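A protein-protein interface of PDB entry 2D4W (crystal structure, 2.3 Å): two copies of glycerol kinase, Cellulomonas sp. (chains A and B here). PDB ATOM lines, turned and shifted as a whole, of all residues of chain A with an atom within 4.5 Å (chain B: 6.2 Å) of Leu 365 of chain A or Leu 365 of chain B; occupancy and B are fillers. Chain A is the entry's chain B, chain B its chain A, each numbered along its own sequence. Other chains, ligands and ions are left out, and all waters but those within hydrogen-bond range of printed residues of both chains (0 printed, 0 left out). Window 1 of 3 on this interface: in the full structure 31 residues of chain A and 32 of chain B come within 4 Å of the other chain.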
ATOM      1  N   ALA A 343     -15.451  -4.413   3.333  1.00  0.00           N
ATOM      2  CA  ALA A 343     -15.679  -5.522   4.266  1.00  0.00           C
ATOM      3  C   ALA A 343     -14.437  -6.064   4.986  1.00  0.00           C
ATOM      4  O   ALA A 343     -13.335  -6.103   4.394  1.00  0.00           O
ATOM      5  CB  ALA A 343     -16.387  -6.644   3.583  1.00  0.00           C
ATOM      6  N   TYR A 344     -14.637  -6.463   6.246  1.00  0.00           N
ATOM      7  CA  TYR A 344     -13.610  -7.030   7.097  1.00  0.00           C
ATOM      8  C   TYR A 344     -14.155  -8.210   7.900  1.00  0.00           C
ATOM      9  O   TYR A 344     -15.241  -8.142   8.501  1.00  0.00           O
ATOM     10  CB  TYR A 344     -13.058  -5.989   8.090  1.00  0.00           C
ATOM     11  CG  TYR A 344     -12.431  -4.772   7.414  1.00  0.00           C
ATOM     12  CD1 TYR A 344     -11.062  -4.683   7.256  1.00  0.00           C
ATOM     13  CD2 TYR A 344     -13.223  -3.728   6.946  1.00  0.00           C
ATOM     14  CE1 TYR A 344     -10.495  -3.597   6.639  1.00  0.00           C
ATOM     15  CE2 TYR A 344     -12.653  -2.622   6.323  1.00  0.00           C
ATOM     16  CZ  TYR A 344     -11.294  -2.574   6.168  1.00  0.00           C
ATOM     17  OH  TYR A 344     -10.718  -1.506   5.538  1.00  0.00           O
ATOM     18  N   PHE A 345     -13.375  -9.290   7.896  1.00  0.00           N
ATOM     19  CA  PHE A 345     -13.685 -10.478   8.649  1.00  0.00           C
ATOM     20  C   PHE A 345     -12.922 -10.456   9.948  1.00  0.00           C
ATOM     21  O   PHE A 345     -11.721 -10.226   9.965  1.00  0.00           O
ATOM     22  CB  PHE A 345     -13.250 -11.748   7.885  1.00  0.00           C
ATOM     23  CG  PHE A 345     -14.345 -12.382   7.069  1.00  0.00           C
ATOM     24  CD1 PHE A 345     -14.219 -12.527   5.692  1.00  0.00           C
ATOM     25  CD2 PHE A 345     -15.502 -12.823   7.679  1.00  0.00           C
ATOM     26  CE1 PHE A 345     -15.230 -13.132   4.946  1.00  0.00           C
ATOM     27  CE2 PHE A 345     -16.519 -13.414   6.946  1.00  0.00           C
ATOM     28  CZ  PHE A 345     -16.397 -13.570   5.582  1.00  0.00           C
ATOM     29  N   ALA A 364     -17.048 -12.309  13.508  1.00  0.00           N
ATOM     30  CA  ALA A 364     -17.953 -11.396  12.852  1.00  0.00           C
ATOM     31  C   ALA A 364     -17.515 -11.048  11.427  1.00  0.00           C
ATOM     32  O   ALA A 364     -16.437 -11.375  10.993  1.00  0.00           O
ATOM     33  CB  ALA A 364     -18.094 -10.087  13.677  1.00  0.00           C
ATOM     34  N   LEU A 365     -18.400 -10.391  10.695  1.00  0.00           N
ATOM     35  CA  LEU A 365     -18.133  -9.899   9.359  1.00  0.00           C
ATOM     36  C   LEU A 365     -18.733  -8.490   9.315  1.00  0.00           C
ATOM     37  O   LEU A 365     -19.967  -8.329   9.417  1.00  0.00           O
ATOM     38  CB  LEU A 365     -18.765 -10.806   8.305  1.00  0.00           C
ATOM     39  CG  LEU A 365     -18.742 -10.286   6.850  1.00  0.00           C
ATOM     40  CD1 LEU A 365     -17.314 -10.060   6.278  1.00  0.00           C
ATOM     41  CD2 LEU A 365     -19.479 -11.222   5.897  1.00  0.00           C
ATOM     42  N   VAL A 366     -17.869  -7.471   9.229  1.00  0.00           N
ATOM     43  CA  VAL A 366     -18.350  -6.089   9.244  1.00  0.00           C
ATOM     44  C   VAL A 366     -18.058  -5.311   7.964  1.00  0.00           C
ATOM     45  O   VAL A 366     -17.300  -5.758   7.098  1.00  0.00           O
ATOM     46  CB  VAL A 366     -17.758  -5.300  10.443  1.00  0.00           C
ATOM     47  CG1 VAL A 366     -17.850  -6.122  11.735  1.00  0.00           C
ATOM     48  CG2 VAL A 366     -16.295  -4.970  10.200  1.00  0.00           C
ATOM     49  N   LEU A 368     -20.451  -4.290   5.765  1.00  0.00           N
ATOM     50  CA  LEU A 368     -21.291  -4.787   4.680  1.00  0.00           C
ATOM     51  C   LEU A 368     -22.181  -3.688   4.153  1.00  0.00           C
ATOM     52  O   LEU A 368     -22.826  -2.988   4.930  1.00  0.00           O
ATOM     53  CB  LEU A 368     -22.186  -5.970   5.142  1.00  0.00           C
ATOM     54  CG  LEU A 368     -21.381  -7.204   5.603  1.00  0.00           C
ATOM     55  CD1 LEU A 368     -22.295  -8.396   5.973  1.00  0.00           C
ATOM     56  CD2 LEU A 368     -20.421  -7.664   4.532  1.00  0.00           C
ATOM     57  N   ILE A 377     -16.025 -10.441  -0.439  1.00  0.00           N
ATOM     58  CA  ILE A 377     -16.009 -11.352   0.713  1.00  0.00           C
ATOM     59  C   ILE A 377     -14.868 -12.326   0.548  1.00  0.00           C
ATOM     60  O   ILE A 377     -14.123 -12.616   1.488  1.00  0.00           O
ATOM     61  CB  ILE A 377     -17.340 -12.106   0.788  1.00  0.00           C
ATOM     62  CG1 ILE A 377     -18.493 -11.111   0.977  1.00  0.00           C
ATOM     63  CG2 ILE A 377     -17.354 -13.118   1.959  1.00  0.00           C
ATOM     64  CD1 ILE A 377     -18.286 -10.192   2.181  1.00  0.00           C
ATOM     65  N   TRP B 316     -30.332  -9.790  -0.829  1.00  0.00           N
ATOM     66  CA  TRP B 316     -28.912  -9.482  -0.995  1.00  0.00           C
ATOM     67  C   TRP B 316     -28.047 -10.737  -0.735  1.00  0.00           C
ATOM     68  O   TRP B 316     -27.055 -10.990  -1.415  1.00  0.00           O
ATOM     69  CB  TRP B 316     -28.535  -8.367   0.000  1.00  0.00           C
ATOM     70  CG  TRP B 316     -27.092  -7.993   0.034  1.00  0.00           C
ATOM     71  CD1 TRP B 316     -26.436  -7.130  -0.829  1.00  0.00           C
ATOM     72  CD2 TRP B 316     -26.107  -8.429   0.983  1.00  0.00           C
ATOM     73  NE1 TRP B 316     -25.116  -7.028  -0.461  1.00  0.00           N
ATOM     74  CE2 TRP B 316     -24.886  -7.824   0.633  1.00  0.00           C
ATOM     75  CE3 TRP B 316     -26.130  -9.298   2.070  1.00  0.00           C
ATOM     76  CZ2 TRP B 316     -23.720  -8.022   1.364  1.00  0.00           C
ATOM     77  CZ3 TRP B 316     -25.000  -9.493   2.784  1.00  0.00           C
ATOM     78  CH2 TRP B 316     -23.789  -8.858   2.436  1.00  0.00           C
ATOM     79  N   LEU B 321     -24.197 -12.560  -2.381  1.00  0.00           N
ATOM     80  CA  LEU B 321     -23.280 -13.548  -1.837  1.00  0.00           C
ATOM     81  C   LEU B 321     -23.461 -14.955  -2.495  1.00  0.00           C
ATOM     82  O   LEU B 321     -22.638 -15.837  -2.305  1.00  0.00           O
ATOM     83  CB  LEU B 321     -23.371 -13.591  -0.321  1.00  0.00           C
ATOM     84  CG  LEU B 321     -23.108 -12.294   0.493  1.00  0.00           C
ATOM     85  CD1 LEU B 321     -22.910 -12.592   1.962  1.00  0.00           C
ATOM     86  CD2 LEU B 321     -21.909 -11.493   0.003  1.00  0.00           C
ATOM     87  N   ALA B 343     -26.029 -16.168  16.113  1.00  0.00           N
ATOM     88  CA  ALA B 343     -25.812 -15.154  15.070  1.00  0.00           C
ATOM     89  C   ALA B 343     -26.828 -14.031  15.121  1.00  0.00           C
ATOM     90  O   ALA B 343     -28.038 -14.277  15.370  1.00  0.00           O
ATOM     91  CB  ALA B 343     -25.866 -15.804  13.658  1.00  0.00           C
ATOM     92  N   TYR B 344     -26.363 -12.821  14.815  1.00  0.00           N
ATOM     93  CA  TYR B 344     -27.230 -11.631  14.729  1.00  0.00           C
ATOM     94  C   TYR B 344     -26.854 -10.786  13.520  1.00  0.00           C
ATOM     95  O   TYR B 344     -25.664 -10.546  13.244  1.00  0.00           O
ATOM     96  CB  TYR B 344     -27.092 -10.755  15.962  1.00  0.00           C
ATOM     97  CG  TYR B 344     -27.574 -11.447  17.227  1.00  0.00           C
ATOM     98  CD1 TYR B 344     -28.876 -11.241  17.699  1.00  0.00           C
ATOM     99  CD2 TYR B 344     -26.729 -12.311  17.939  1.00  0.00           C
ATOM    100  CE1 TYR B 344     -29.330 -11.884  18.856  1.00  0.00           C
ATOM    101  CE2 TYR B 344     -27.174 -12.959  19.098  1.00  0.00           C
ATOM    102  CZ  TYR B 344     -28.477 -12.740  19.544  1.00  0.00           C
ATOM    103  OH  TYR B 344     -28.924 -13.377  20.683  1.00  0.00           O
ATOM    104  N   PHE B 345     -27.879 -10.322  12.813  1.00  0.00           N
ATOM    105  CA  PHE B 345     -27.694  -9.470  11.654  1.00  0.00           C
ATOM    106  C   PHE B 345     -27.983  -8.020  12.033  1.00  0.00           C
ATOM    107  O   PHE B 345     -29.083  -7.692  12.506  1.00  0.00           O
ATOM    108  CB  PHE B 345     -28.669  -9.847  10.559  1.00  0.00           C
ATOM    109  CG  PHE B 345     -28.050 -10.630   9.432  1.00  0.00           C
ATOM    110  CD1 PHE B 345     -28.451 -11.940   9.140  1.00  0.00           C
ATOM    111  CD2 PHE B 345     -27.046 -10.069   8.679  1.00  0.00           C
ATOM    112  CE1 PHE B 345     -27.847 -12.665   8.086  1.00  0.00           C
ATOM    113  CE2 PHE B 345     -26.478 -10.750   7.650  1.00  0.00           C
ATOM    114  CZ  PHE B 345     -26.872 -12.048   7.336  1.00  0.00           C
ATOM    115  N   VAL B 346     -26.992  -7.169  11.801  1.00  0.00           N
ATOM    116  CA  VAL B 346     -27.118  -5.740  12.026  1.00  0.00           C
ATOM    117  C   VAL B 346     -27.337  -5.137  10.674  1.00  0.00           C
ATOM    118  O   VAL B 346     -26.390  -4.699  10.039  1.00  0.00           O
ATOM    119  CB  VAL B 346     -25.815  -5.168  12.656  1.00  0.00           C
ATOM    120  CG1 VAL B 346     -25.803  -3.639  12.643  1.00  0.00           C
ATOM    121  CG2 VAL B 346     -25.667  -5.657  14.112  1.00  0.00           C
ATOM    122  N   GLY B 363     -23.493  -2.235   7.596  1.00  0.00           N
ATOM    123  CA  GLY B 363     -24.079  -3.234   8.463  1.00  0.00           C
ATOM    124  C   GLY B 363     -23.036  -4.296   8.810  1.00  0.00           C
ATOM    125  O   GLY B 363     -21.862  -4.195   8.411  1.00  0.00           O
ATOM    126  N   ALA B 364     -23.463  -5.333   9.534  1.00  0.00           N
ATOM    127  CA  ALA B 364     -22.589  -6.380   9.963  1.00  0.00           C
ATOM    128  C   ALA B 364     -23.371  -7.654  10.274  1.00  0.00           C
ATOM    129  O   ALA B 364     -24.602  -7.687  10.255  1.00  0.00           O
ATOM    130  CB  ALA B 364     -21.803  -5.945  11.211  1.00  0.00           C
ATOM    131  N   LEU B 365     -22.611  -8.700  10.571  1.00  0.00           N
ATOM    132  CA  LEU B 365     -23.109 -10.029  10.970  1.00  0.00           C
ATOM    133  C   LEU B 365     -22.181 -10.505  12.073  1.00  0.00           C
ATOM    134  O   LEU B 365     -21.007 -10.702  11.825  1.00  0.00           O
ATOM    135  CB  LEU B 365     -23.114 -11.000   9.780  1.00  0.00           C
ATOM    136  CG  LEU B 365     -23.280 -12.523  10.061  1.00  0.00           C
ATOM    137  CD1 LEU B 365     -24.662 -12.635  10.696  1.00  0.00           C
ATOM    138  CD2 LEU B 365     -23.211 -13.308   8.753  1.00  0.00           C
ATOM    139  N   VAL B 366     -22.697 -10.612  13.290  1.00  0.00           N
ATOM    140  CA  VAL B 366     -21.874 -10.972  14.448  1.00  0.00           C
ATOM    141  C   VAL B 366     -22.339 -12.300  15.020  1.00  0.00           C
ATOM    142  O   VAL B 366     -23.426 -12.779  14.695  1.00  0.00           O
ATOM    143  CB  VAL B 366     -21.957  -9.885  15.538  1.00  0.00           C
ATOM    144  CG1 VAL B 366     -21.551  -8.544  14.986  1.00  0.00           C
ATOM    145  CG2 VAL B 366     -23.390  -9.774  16.105  1.00  0.00           C
ATOM    146  N   GLY B 367     -21.516 -12.877  15.893  1.00  0.00           N
ATOM    147  CA  GLY B 367     -21.826 -14.145  16.527  1.00  0.00           C
ATOM    148  C   GLY B 367     -21.618 -15.390  15.702  1.00  0.00           C
ATOM    149  O   GLY B 367     -22.334 -16.362  15.879  1.00  0.00           O
ATOM    150  N   LEU B 368     -20.628 -15.380  14.820  1.00  0.00           N
ATOM    151  CA  LEU B 368     -20.326 -16.542  14.011  1.00  0.00           C
ATOM    152  C   LEU B 368     -19.379 -17.482  14.755  1.00  0.00           C
ATOM    153  O   LEU B 368     -18.343 -17.040  15.280  1.00  0.00           O
ATOM    154  CB  LEU B 368     -19.625 -16.131  12.721  1.00  0.00           C
ATOM    155  CG  LEU B 368     -20.328 -15.003  11.949  1.00  0.00           C
ATOM    156  CD1 LEU B 368     -19.646 -14.651  10.609  1.00  0.00           C
ATOM    157  CD2 LEU B 368     -21.793 -15.357  11.732  1.00  0.00           C
ATOM    158  N   ILE B 377     -28.229 -18.543   9.680  1.00  0.00           N
ATOM    159  CA  ILE B 377     -28.147 -17.269   8.987  1.00  0.00           C
ATOM    160  C   ILE B 377     -29.527 -16.887   8.419  1.00  0.00           C
ATOM    161  O   ILE B 377     -29.921 -15.728   8.494  1.00  0.00           O
ATOM    162  CB  ILE B 377     -27.091 -17.344   7.862  1.00  0.00           C
ATOM    163  CG1 ILE B 377     -25.693 -17.582   8.438  1.00  0.00           C
ATOM    164  CG2 ILE B 377     -27.119 -16.105   7.033  1.00  0.00           C
ATOM    165  CD1 ILE B 377     -25.376 -16.780   9.695  1.00  0.00           C
ATOM    166  N   ALA B 380     -31.497 -15.781  11.463  1.00  0.00           N
ATOM    167  CA  ALA B 380     -31.107 -14.446  11.944  1.00  0.00           C
ATOM    168  C   ALA B 380     -31.528 -13.335  10.974  1.00  0.00           C
ATOM    169  O   ALA B 380     -31.841 -12.211  11.346  1.00  0.00           O
ATOM    170  CB  ALA B 380     -29.669 -14.386  12.173  1.00  0.00           C
ATOM    171  N   THR B 494     -21.705  -2.085  16.372  1.00  0.00           N
ATOM    172  CA  THR B 494     -21.483  -1.940  14.947  1.00  0.00           C
ATOM    173  C   THR B 494     -21.386  -0.450  14.586  1.00  0.00           C
ATOM    174  O   THR B 494     -20.581  -0.062  13.761  1.00  0.00           O
ATOM    175  CB  THR B 494     -22.624  -2.580  14.154  1.00  0.00           C
ATOM    176  OG1 THR B 494     -22.542  -3.995  14.274  1.00  0.00           O
ATOM    177  CG2 THR B 494     -22.404  -2.345  12.635  1.00  0.00           C
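Printed residues of chain B that touch a printed residue of chain A: Trp 316, Leu 321, Gly 363, Ala 364, Leu 365 and Val 366. Hydrophobic or aromatic side chains of chain B that line the printed part of chain A: Trp 316, Leu 321 and Ala 364. Along chain B the printed residues that touch a printed residue of chain A span positions 316 to 366. Hydrophobic or aromatic side chains of chain A within 4 Å of the printed part of chain B: Ala 364, Val 366, Leu 368 and Ile 377. Along chain A the printed residues that touch a printed residue of chain B span positions 364 to 377.
Ala 364 of chain A touches Leu 365 of chain B, and with the chains exchanged Leu 365 of chain A touches Ala 364 of chain B. Ala 364 of chain A touches Val 366 of chain B, and with the chains exchanged Val 366 of chain A touches Ala 364 of chain B. Leu 365 of chain B touches its own counterpart, Leu 365 of chain A. 8 positions are printed for both chains. Of the 9 pairs that touch across the chains among the printed residues, 5 have their exchanged pair printed and touching as well.
O of Tyr 344 of chain A is in hydrogen-bond range of N of Val 366 of chain A (2.8 Å). The backbone carbonyl oxygen (O) of Val 366 of chain B is in hydrogen-bond range of the backbone NH (N) of Tyr 344 of chain B (2.9 Å). The backbone NH (N) of Leu 321 of chain B is in hydrogen-bond range of the backbone carbonyl oxygen (O) of Trp 316 of chain B (3.4 Å). The backbone NH of Val 346 of chain B is in hydrogen-bond range of the backbone carbonyl oxygen of Ala 364 of chain B (2.9 Å).
Leu 365 of chain B touches Ala 364 of chain A. Val 366 of chain B touches Ala 364 of chain A (CA to CB, 3.96 Å). O of Leu 365 of chain A touches CA of Ala 364 of chain B (3.3 Å). Val 366 of chain A touches Gly 363 of chain B. Ala 364 of chain B touches Val 366 of chain A (CB to CA, 3.98 Å). Leu 368 of chain A touches Trp 316 of chain B. Ile 377 of chain A touches Leu 321 of chain B.
Leu 365 of chain A touches just these residues of chain B: Ala 364 (3.3 Å) and Leu 365 (2.9 Å). Of chain A, only Ala 364 and Leu 365 come within 4 Å of Leu 365 of chain B. Of the printed residues of chain A, Gly 363 of chain B touches Val 366 and Leu 368. Printed residues of chain B within 4 Å of Ile 377 of chain A: Leu 321. Of the printed residues of chain B, Ala 364 of chain A touches Leu 365 and Val 366. Of the printed residues of chain B, Val 366 of chain A touches Gly 363 (3.99 Å) and Ala 364 (3.98 Å). The nearest printed residue of chain A that does not touch Leu 365 of chain B is Leu 368 of chain A (4.6 Å).
The backbone NH of Gly 363 of chain B lies within hydrogen-bond range of the backbone carbonyl oxygen of Leu 368 of chain A (2.8 Å). The backbone NH (N) of Leu 365 of chain A sits at hydrogen-bond distance from the backbone carbonyl oxygen (O) of Leu 365 of chain B, at 2.9 Å.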
